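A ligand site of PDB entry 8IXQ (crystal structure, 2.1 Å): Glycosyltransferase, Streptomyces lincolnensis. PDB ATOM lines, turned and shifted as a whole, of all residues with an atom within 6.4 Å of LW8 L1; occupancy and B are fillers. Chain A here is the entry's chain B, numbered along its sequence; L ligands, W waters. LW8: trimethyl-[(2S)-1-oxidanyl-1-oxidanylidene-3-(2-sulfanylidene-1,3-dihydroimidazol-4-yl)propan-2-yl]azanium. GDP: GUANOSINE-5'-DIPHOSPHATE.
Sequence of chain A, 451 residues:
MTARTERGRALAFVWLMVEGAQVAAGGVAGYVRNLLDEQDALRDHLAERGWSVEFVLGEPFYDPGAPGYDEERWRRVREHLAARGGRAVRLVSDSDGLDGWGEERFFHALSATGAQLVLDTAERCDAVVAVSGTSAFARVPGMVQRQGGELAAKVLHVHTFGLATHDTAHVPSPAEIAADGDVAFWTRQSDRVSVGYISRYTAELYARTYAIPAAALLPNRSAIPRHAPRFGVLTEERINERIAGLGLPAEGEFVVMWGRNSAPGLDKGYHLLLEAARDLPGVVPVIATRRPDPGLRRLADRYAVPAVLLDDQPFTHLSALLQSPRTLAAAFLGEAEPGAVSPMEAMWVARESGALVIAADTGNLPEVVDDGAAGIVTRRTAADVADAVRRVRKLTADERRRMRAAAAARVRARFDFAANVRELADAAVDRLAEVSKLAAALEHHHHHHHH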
ATOM      1  N   VAL A  18      -8.884   1.138  12.665  1.00  0.00           N
ATOM      2  CA  VAL A  18      -9.267   2.094  11.642  1.00  0.00           C
ATOM      3  C   VAL A  18      -9.481   3.490  12.205  1.00  0.00           C
ATOM      4  O   VAL A  18      -9.491   4.475  11.441  1.00  0.00           O
ATOM      5  CB  VAL A  18     -10.527   1.618  10.875  1.00  0.00           C
ATOM      6  CG1 VAL A  18     -10.236   0.309  10.123  1.00  0.00           C
ATOM      7  CG2 VAL A  18     -11.721   1.456  11.833  1.00  0.00           C
ATOM      8  N   GLU A  19      -9.606   3.608  13.524  1.00  0.00           N
ATOM      9  CA  GLU A  19      -9.702   4.907  14.183  1.00  0.00           C
ATOM     10  C   GLU A  19      -9.196   4.730  15.615  1.00  0.00           C
ATOM     11  O   GLU A  19      -8.933   3.611  16.062  1.00  0.00           O
ATOM     12  CB  GLU A  19     -11.144   5.454  14.146  1.00  0.00           C
ATOM     13  CG  GLU A  19     -12.119   4.523  14.823  1.00  0.00           C
ATOM     14  CD  GLU A  19     -13.426   5.184  15.265  1.00  0.00           C
ATOM     15  OE1 GLU A  19     -13.687   6.364  14.910  1.00  0.00           O
ATOM     16  OE2 GLU A  19     -14.185   4.501  15.997  1.00  0.00           O
ATOM     17  N   GLY A  27     -17.105   2.786  18.233  1.00  0.00           N
ATOM     18  CA  GLY A  27     -16.656   1.789  19.194  1.00  0.00           C
ATOM     19  C   GLY A  27     -15.201   1.387  19.044  1.00  0.00           C
ATOM     20  O   GLY A  27     -14.535   1.068  20.025  1.00  0.00           O
ATOM     21  N   VAL A  28     -14.685   1.387  17.807  1.00  0.00           N
ATOM     22  CA  VAL A  28     -13.274   1.057  17.595  1.00  0.00           C
ATOM     23  C   VAL A  28     -12.399   2.081  18.302  1.00  0.00           C
ATOM     24  O   VAL A  28     -11.461   1.721  19.021  1.00  0.00           O
ATOM     25  CB  VAL A  28     -12.950   0.979  16.085  1.00  0.00           C
ATOM     26  CG1 VAL A  28     -11.426   0.918  15.850  1.00  0.00           C
ATOM     27  CG2 VAL A  28     -13.619  -0.239  15.449  1.00  0.00           C
ATOM     28  N   GLY A 100     -12.558   7.002   7.255  1.00  0.00           N
ATOM     29  CA  GLY A 100     -11.943   5.816   7.828  1.00  0.00           C
ATOM     30  C   GLY A 100     -12.453   4.509   7.251  1.00  0.00           C
ATOM     31  O   GLY A 100     -12.442   3.484   7.941  1.00  0.00           O
ATOM     32  N   TRP A 101     -12.891   4.543   5.988  1.00  0.00           N
ATOM     33  CA  TRP A 101     -13.369   3.367   5.278  1.00  0.00           C
ATOM     34  C   TRP A 101     -13.084   3.565   3.798  1.00  0.00           C
ATOM     35  O   TRP A 101     -12.590   4.611   3.374  1.00  0.00           O
ATOM     36  CB  TRP A 101     -14.869   3.133   5.529  1.00  0.00           C
ATOM     37  CG  TRP A 101     -15.281   1.689   5.367  1.00  0.00           C
ATOM     38  CD1 TRP A 101     -16.086   1.154   4.397  1.00  0.00           C
ATOM     39  CD2 TRP A 101     -14.880   0.601   6.203  1.00  0.00           C
ATOM     40  NE1 TRP A 101     -16.206  -0.211   4.582  1.00  0.00           N
ATOM     41  CE2 TRP A 101     -15.477  -0.570   5.682  1.00  0.00           C
ATOM     42  CE3 TRP A 101     -14.064   0.494   7.337  1.00  0.00           C
ATOM     43  CZ2 TRP A 101     -15.299  -1.829   6.271  1.00  0.00           C
ATOM     44  CZ3 TRP A 101     -13.891  -0.757   7.927  1.00  0.00           C
ATOM     45  CH2 TRP A 101     -14.499  -1.904   7.382  1.00  0.00           C
ATOM     46  N   THR A 134     -11.812  -5.096  11.841  1.00  0.00           N
ATOM     47  CA  THR A 134     -12.733  -4.798  10.739  1.00  0.00           C
ATOM     48  C   THR A 134     -12.221  -5.327   9.400  1.00  0.00           C
ATOM     49  O   THR A 134     -11.053  -5.693   9.266  1.00  0.00           O
ATOM     50  CB  THR A 134     -13.049  -3.292  10.608  1.00  0.00           C
ATOM     51  OG1 THR A 134     -12.021  -2.640   9.847  1.00  0.00           O
ATOM     52  CG2 THR A 134     -13.244  -2.592  11.972  1.00  0.00           C
ATOM     53  N   SER A 135     -13.119  -5.379   8.398  1.00  0.00           N
ATOM     54  CA  SER A 135     -12.762  -5.908   7.089  1.00  0.00           C
ATOM     55  C   SER A 135     -11.577  -5.189   6.471  1.00  0.00           C
ATOM     56  O   SER A 135     -10.844  -5.780   5.663  1.00  0.00           O
ATOM     57  CB  SER A 135     -13.967  -5.816   6.133  1.00  0.00           C
ATOM     58  OG  SER A 135     -15.136  -6.326   6.750  1.00  0.00           O
ATOM     59  N   PHE A 161     -13.669  -7.638  15.372  1.00  0.00           N
ATOM     60  CA  PHE A 161     -14.619  -6.562  15.063  1.00  0.00           C
ATOM     61  C   PHE A 161     -15.496  -6.881  13.852  1.00  0.00           C
ATOM     62  O   PHE A 161     -15.566  -8.033  13.413  1.00  0.00           O
ATOM     63  CB  PHE A 161     -13.901  -5.211  14.863  1.00  0.00           C
ATOM     64  CG  PHE A 161     -13.116  -4.753  16.065  1.00  0.00           C
ATOM     65  CD1 PHE A 161     -13.349  -5.301  17.317  1.00  0.00           C
ATOM     66  CD2 PHE A 161     -12.124  -3.793  15.942  1.00  0.00           C
ATOM     67  CE1 PHE A 161     -12.635  -4.895  18.417  1.00  0.00           C
ATOM     68  CE2 PHE A 161     -11.409  -3.374  17.038  1.00  0.00           C
ATOM     69  CZ  PHE A 161     -11.661  -3.930  18.282  1.00  0.00           C
ATOM     70  N   GLY A 162     -16.147  -5.853  13.314  1.00  0.00           N
ATOM     71  CA  GLY A 162     -17.233  -6.069  12.360  1.00  0.00           C
ATOM     72  C   GLY A 162     -16.762  -6.671  11.037  1.00  0.00           C
ATOM     73  O   GLY A 162     -15.608  -6.523  10.627  1.00  0.00           O
ATOM     74  N   LEU A 163     -17.698  -7.337  10.357  1.00  0.00           N
ATOM     75  CA  LEU A 163     -17.388  -8.150   9.194  1.00  0.00           C
ATOM     76  C   LEU A 163     -18.608  -8.242   8.288  1.00  0.00           C
ATOM     77  O   LEU A 163     -19.720  -7.856   8.669  1.00  0.00           O
ATOM     78  CB  LEU A 163     -16.918  -9.553   9.599  1.00  0.00           C
ATOM     79  CG  LEU A 163     -17.975 -10.515  10.166  1.00  0.00           C
ATOM     80  CD1 LEU A 163     -17.369 -11.936  10.329  1.00  0.00           C
ATOM     81  CD2 LEU A 163     -18.595 -10.027  11.518  1.00  0.00           C
ATOM     82  N   GLU A 176     -15.500  -5.897   1.218  1.00  0.00           N
ATOM     83  CA  GLU A 176     -15.746  -6.486   2.519  1.00  0.00           C
ATOM     84  C   GLU A 176     -15.927  -7.988   2.398  1.00  0.00           C
ATOM     85  O   GLU A 176     -15.356  -8.749   3.198  1.00  0.00           O
ATOM     86  CB  GLU A 176     -16.979  -5.835   3.172  1.00  0.00           C
ATOM     87  CG  GLU A 176     -16.732  -4.386   3.619  1.00  0.00           C
ATOM     88  CD  GLU A 176     -17.993  -3.503   3.533  1.00  0.00           C
ATOM     89  OE1 GLU A 176     -19.105  -4.050   3.655  1.00  0.00           O
ATOM     90  OE2 GLU A 176     -17.863  -2.274   3.348  1.00  0.00           O
ATOM     91  N   ILE A 198     -16.290 -10.846  19.552  1.00  0.00           N
ATOM     92  CA  ILE A 198     -16.615  -9.742  20.443  1.00  0.00           C
ATOM     93  C   ILE A 198     -17.950  -9.956  21.146  1.00  0.00           C
ATOM     94  O   ILE A 198     -18.313  -9.166  22.032  1.00  0.00           O
ATOM     95  CB  ILE A 198     -16.622  -8.394  19.690  1.00  0.00           C
ATOM     96  CG1 ILE A 198     -17.673  -8.390  18.578  1.00  0.00           C
ATOM     97  CG2 ILE A 198     -15.229  -8.120  19.113  1.00  0.00           C
ATOM     98  CD1 ILE A 198     -17.706  -7.093  17.779  1.00  0.00           C
ATOM     99  N   ARG A 260     -22.967   7.177  16.298  1.00  0.00           N
ATOM    100  CA  ARG A 260     -22.636   7.573  14.930  1.00  0.00           C
ATOM    101  C   ARG A 260     -23.911   7.677  14.104  1.00  0.00           C
ATOM    102  O   ARG A 260     -24.847   6.891  14.267  1.00  0.00           O
ATOM    103  CB  ARG A 260     -21.689   6.559  14.290  1.00  0.00           C
ATOM    104  CG  ARG A 260     -20.302   6.550  14.934  1.00  0.00           C
ATOM    105  CD  ARG A 260     -19.340   5.670  14.162  1.00  0.00           C
ATOM    106  NE  ARG A 260     -19.721   4.260  14.266  1.00  0.00           N
ATOM    107  CZ  ARG A 260     -19.597   3.384  13.274  1.00  0.00           C
ATOM    108  NH1 ARG A 260     -19.079   3.743  12.104  1.00  0.00           N
ATOM    109  NH2 ARG A 260     -19.986   2.115  13.458  1.00  0.00           N
ATOM    110  N   ALA A 263     -25.735   5.363   8.248  1.00  0.00           N
ATOM    111  CA  ALA A 263     -25.094   5.495   6.945  1.00  0.00           C
ATOM    112  C   ALA A 263     -25.292   4.178   6.211  1.00  0.00           C
ATOM    113  O   ALA A 263     -25.806   3.211   6.798  1.00  0.00           O
ATOM    114  CB  ALA A 263     -23.596   5.852   7.102  1.00  0.00           C
ATOM    115  N   PRO A 264     -24.916   4.098   4.930  1.00  0.00           N
ATOM    116  CA  PRO A 264     -25.020   2.814   4.227  1.00  0.00           C
ATOM    117  C   PRO A 264     -24.225   1.714   4.915  1.00  0.00           C
ATOM    118  O   PRO A 264     -23.040   1.887   5.254  1.00  0.00           O
ATOM    119  CB  PRO A 264     -24.459   3.147   2.833  1.00  0.00           C
ATOM    120  CG  PRO A 264     -24.881   4.573   2.639  1.00  0.00           C
ATOM    121  CD  PRO A 264     -24.709   5.221   4.002  1.00  0.00           C
ATOM    122  N   GLY A 265     -24.881   0.587   5.151  1.00  0.00           N
ATOM    123  CA  GLY A 265     -24.269  -0.482   5.915  1.00  0.00           C
ATOM    124  C   GLY A 265     -24.301  -0.287   7.418  1.00  0.00           C
ATOM    125  O   GLY A 265     -23.823  -1.167   8.156  1.00  0.00           O
ATOM    126  N   LEU A 266     -24.889   0.823   7.913  1.00  0.00           N
ATOM    127  CA  LEU A 266     -24.899   1.119   9.343  1.00  0.00           C
ATOM    128  C   LEU A 266     -26.251   1.772   9.663  1.00  0.00           C
ATOM    129  O   LEU A 266     -26.379   2.999   9.766  1.00  0.00           O
ATOM    130  CB  LEU A 266     -23.729   2.021   9.733  1.00  0.00           C
ATOM    131  CG  LEU A 266     -23.491   2.253  11.229  1.00  0.00           C
ATOM    132  CD1 LEU A 266     -22.970   0.993  11.893  1.00  0.00           C
ATOM    133  CD2 LEU A 266     -22.540   3.429  11.429  1.00  0.00           C
ATOM    134  N   PRO A 338     -22.441  -5.849  15.488  1.00  0.00           N
ATOM    135  CA  PRO A 338     -21.589  -7.001  15.837  1.00  0.00           C
ATOM    136  C   PRO A 338     -21.253  -7.050  17.320  1.00  0.00           C
ATOM    137  O   PRO A 338     -21.149  -8.156  17.879  1.00  0.00           O
ATOM    138  CB  PRO A 338     -20.345  -6.808  14.962  1.00  0.00           C
ATOM    139  CG  PRO A 338     -20.347  -5.319  14.606  1.00  0.00           C
ATOM    140  CD  PRO A 338     -21.812  -4.947  14.512  1.00  0.00           C
HETATM  141  O01 LW8 L   1     -19.927   0.223  11.079  1.00  0.00           O
HETATM  142  C02 LW8 L   1     -19.240   0.662  10.119  1.00  0.00           C
HETATM  143  O03 LW8 L   1     -19.013   1.866   9.880  1.00  0.00           O
HETATM  144  C04 LW8 L   1     -18.576  -0.396   9.196  1.00  0.00           C
HETATM  145  N05 LW8 L   1     -19.071  -0.315   7.794  1.00  0.00           N
HETATM  146  C06 LW8 L   1     -18.787  -1.610   7.169  1.00  0.00           C
HETATM  147  C07 LW8 L   1     -20.530  -0.110   7.780  1.00  0.00           C
HETATM  148  C08 LW8 L   1     -18.439   0.768   7.001  1.00  0.00           C
HETATM  149  C09 LW8 L   1     -17.036  -0.283   9.395  1.00  0.00           C
HETATM  150  C10 LW8 L   1     -16.843  -0.500  10.901  1.00  0.00           C
HETATM  151  N11 LW8 L   1     -17.000  -1.679  11.496  1.00  0.00           N
HETATM  152  C14 LW8 L   1     -16.786  -1.470  12.786  1.00  0.00           C
HETATM  153  S15 LW8 L   1     -16.892  -2.767  14.041  1.00  0.00           S
HETATM  154  N13 LW8 L   1     -16.508  -0.187  13.016  1.00  0.00           N
HETATM  155  C12 LW8 L   1     -16.554   0.438  11.818  1.00  0.00           C
HETATM  156  PB  GDP L   2     -20.207   1.585  16.962  1.00  0.00           P
HETATM  157  O1B GDP L   2     -19.936   3.070  16.923  1.00  0.00           O
HETATM  158  O2B GDP L   2     -21.148   1.135  15.857  1.00  0.00           O
HETATM  159  O3B GDP L   2     -18.936   0.789  17.152  1.00  0.00           O
HETATM  160  O3A GDP L   2     -21.126   1.339  18.286  1.00  0.00           O
HETATM  161  PA  GDP L   2     -20.711   1.109  19.828  1.00  0.00           P
HETATM  162  O1A GDP L   2     -20.029  -0.234  20.038  1.00  0.00           O
HETATM  163  O2A GDP L   2     -21.924   1.486  20.646  1.00  0.00           O
HETATM  164  O5' GDP L   2     -19.616   2.232  20.145  1.00  0.00           O
HETATM  165  C5' GDP L   2     -19.964   3.606  20.147  1.00  0.00           C
HETATM  166  C4' GDP L   2     -18.982   4.292  21.096  1.00  0.00           C
HETATM  167  O4' GDP L   2     -18.862   5.651  20.692  1.00  0.00           O
HETATM  168  C3' GDP L   2     -19.603   4.291  22.483  1.00  0.00           C
HETATM  169  O3' GDP L   2     -18.541   4.402  23.431  1.00  0.00           O
HETATM  170  C2' GDP L   2     -20.386   5.579  22.462  1.00  0.00           C
HETATM  171  O2' GDP L   2     -20.637   6.059  23.784  1.00  0.00           O
HETATM  172  C1' GDP L   2     -19.450   6.488  21.688  1.00  0.00           C
HETATM  173  N9  GDP L   2     -20.250   7.562  21.052  1.00  0.00           N
HETATM  174  C8  GDP L   2     -20.964   7.408  19.924  1.00  0.00           C
HETATM  175  N7  GDP L   2     -21.605   8.557  19.591  1.00  0.00           N
HETATM  176  C5  GDP L   2     -21.283   9.462  20.528  1.00  0.00           C
HETATM  177  C6  GDP L   2     -21.609  10.875  20.761  1.00  0.00           C
HETATM  178  O6  GDP L   2     -22.369  11.492  19.977  1.00  0.00           O
HETATM  179  N1  GDP L   2     -21.064  11.460  21.843  1.00  0.00           N
HETATM  180  C2  GDP L   2     -20.239  10.804  22.702  1.00  0.00           C
HETATM  181  N2  GDP L   2     -19.723  11.459  23.765  1.00  0.00           N
HETATM  182  N3  GDP L   2     -19.885   9.495  22.540  1.00  0.00           N
HETATM  183  C4  GDP L   2     -20.376   8.794  21.481  1.00  0.00           C
HETATM  184  O   HOH W   1     -16.285   3.096   9.268  1.00  0.00           O
HETATM  185  O   HOH W   2     -20.745  -1.935  12.259  1.00  0.00           O
HETATM  186  O   HOH W   3     -19.788  -1.934  15.229  1.00  0.00           O
HETATM  187  O   HOH W   4     -20.732   0.098   4.580  1.00  0.00           O
HETATM  188  O   HOH W   5     -20.403   3.838   8.313  1.00  0.00           O
HETATM  189  O   HOH W   6     -17.231  -4.599   7.400  1.00  0.00           O
HETATM  190  O   HOH W   7     -17.766  -3.813   9.763  1.00  0.00           O
HETATM  191  O   HOH W   8     -16.726   1.140  15.525  1.00  0.00           O
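The backbone NH (N) of Gly 162 lies close to a sulfur (S15) of LW8 L1, 3.3 Å away.
The backbone NH (N) of Gly 27 sits at hydrogen-bond distance from an oxygen (O3B) of GDP L2, 2.9 Å away.
An oxygen (O2B) of GDP L2 is in salt-bridge range of the guanidinium group (NH2) of Arg 260 (2.8 Å).
NH1 of Arg 260 is in salt-bridge range of O03 of LW8 L1 (2.9 Å).
The side-chain carboxylate (OE2) of Glu 176 lies within hydrogen-bond range of the indole nitrogen (NE1) of Trp 101 (2.9 Å).
CG2 of Val 28 touches N13 of LW8 L1 (3.8 Å).
NE1 of Trp 101 touches C08 of LW8 L1, at 3.4 Å.
CG2 of Thr 134 touches C14 of LW8 L1, 3.8 Å away.
Phe 161 touches LW8 L1.
Glu 176 touches LW8 L1.
Gly 265 touches LW8 L1.
Leu 266 touches LW8 L1.
Within 4 Å of LW8 L1: Val 28, Trp 101, Thr 134, Phe 161, Gly 162, Glu 176, Arg 260, Gly 265 and Leu 266.
The nearest printed residue that does not touch LW8 L1 is Pro 264 (4.1 Å).
Water W3 lies within hydrogen-bond range of S15 of LW8 L1 (3.2 Å) and O2B of GDP L2 (3.4 Å).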
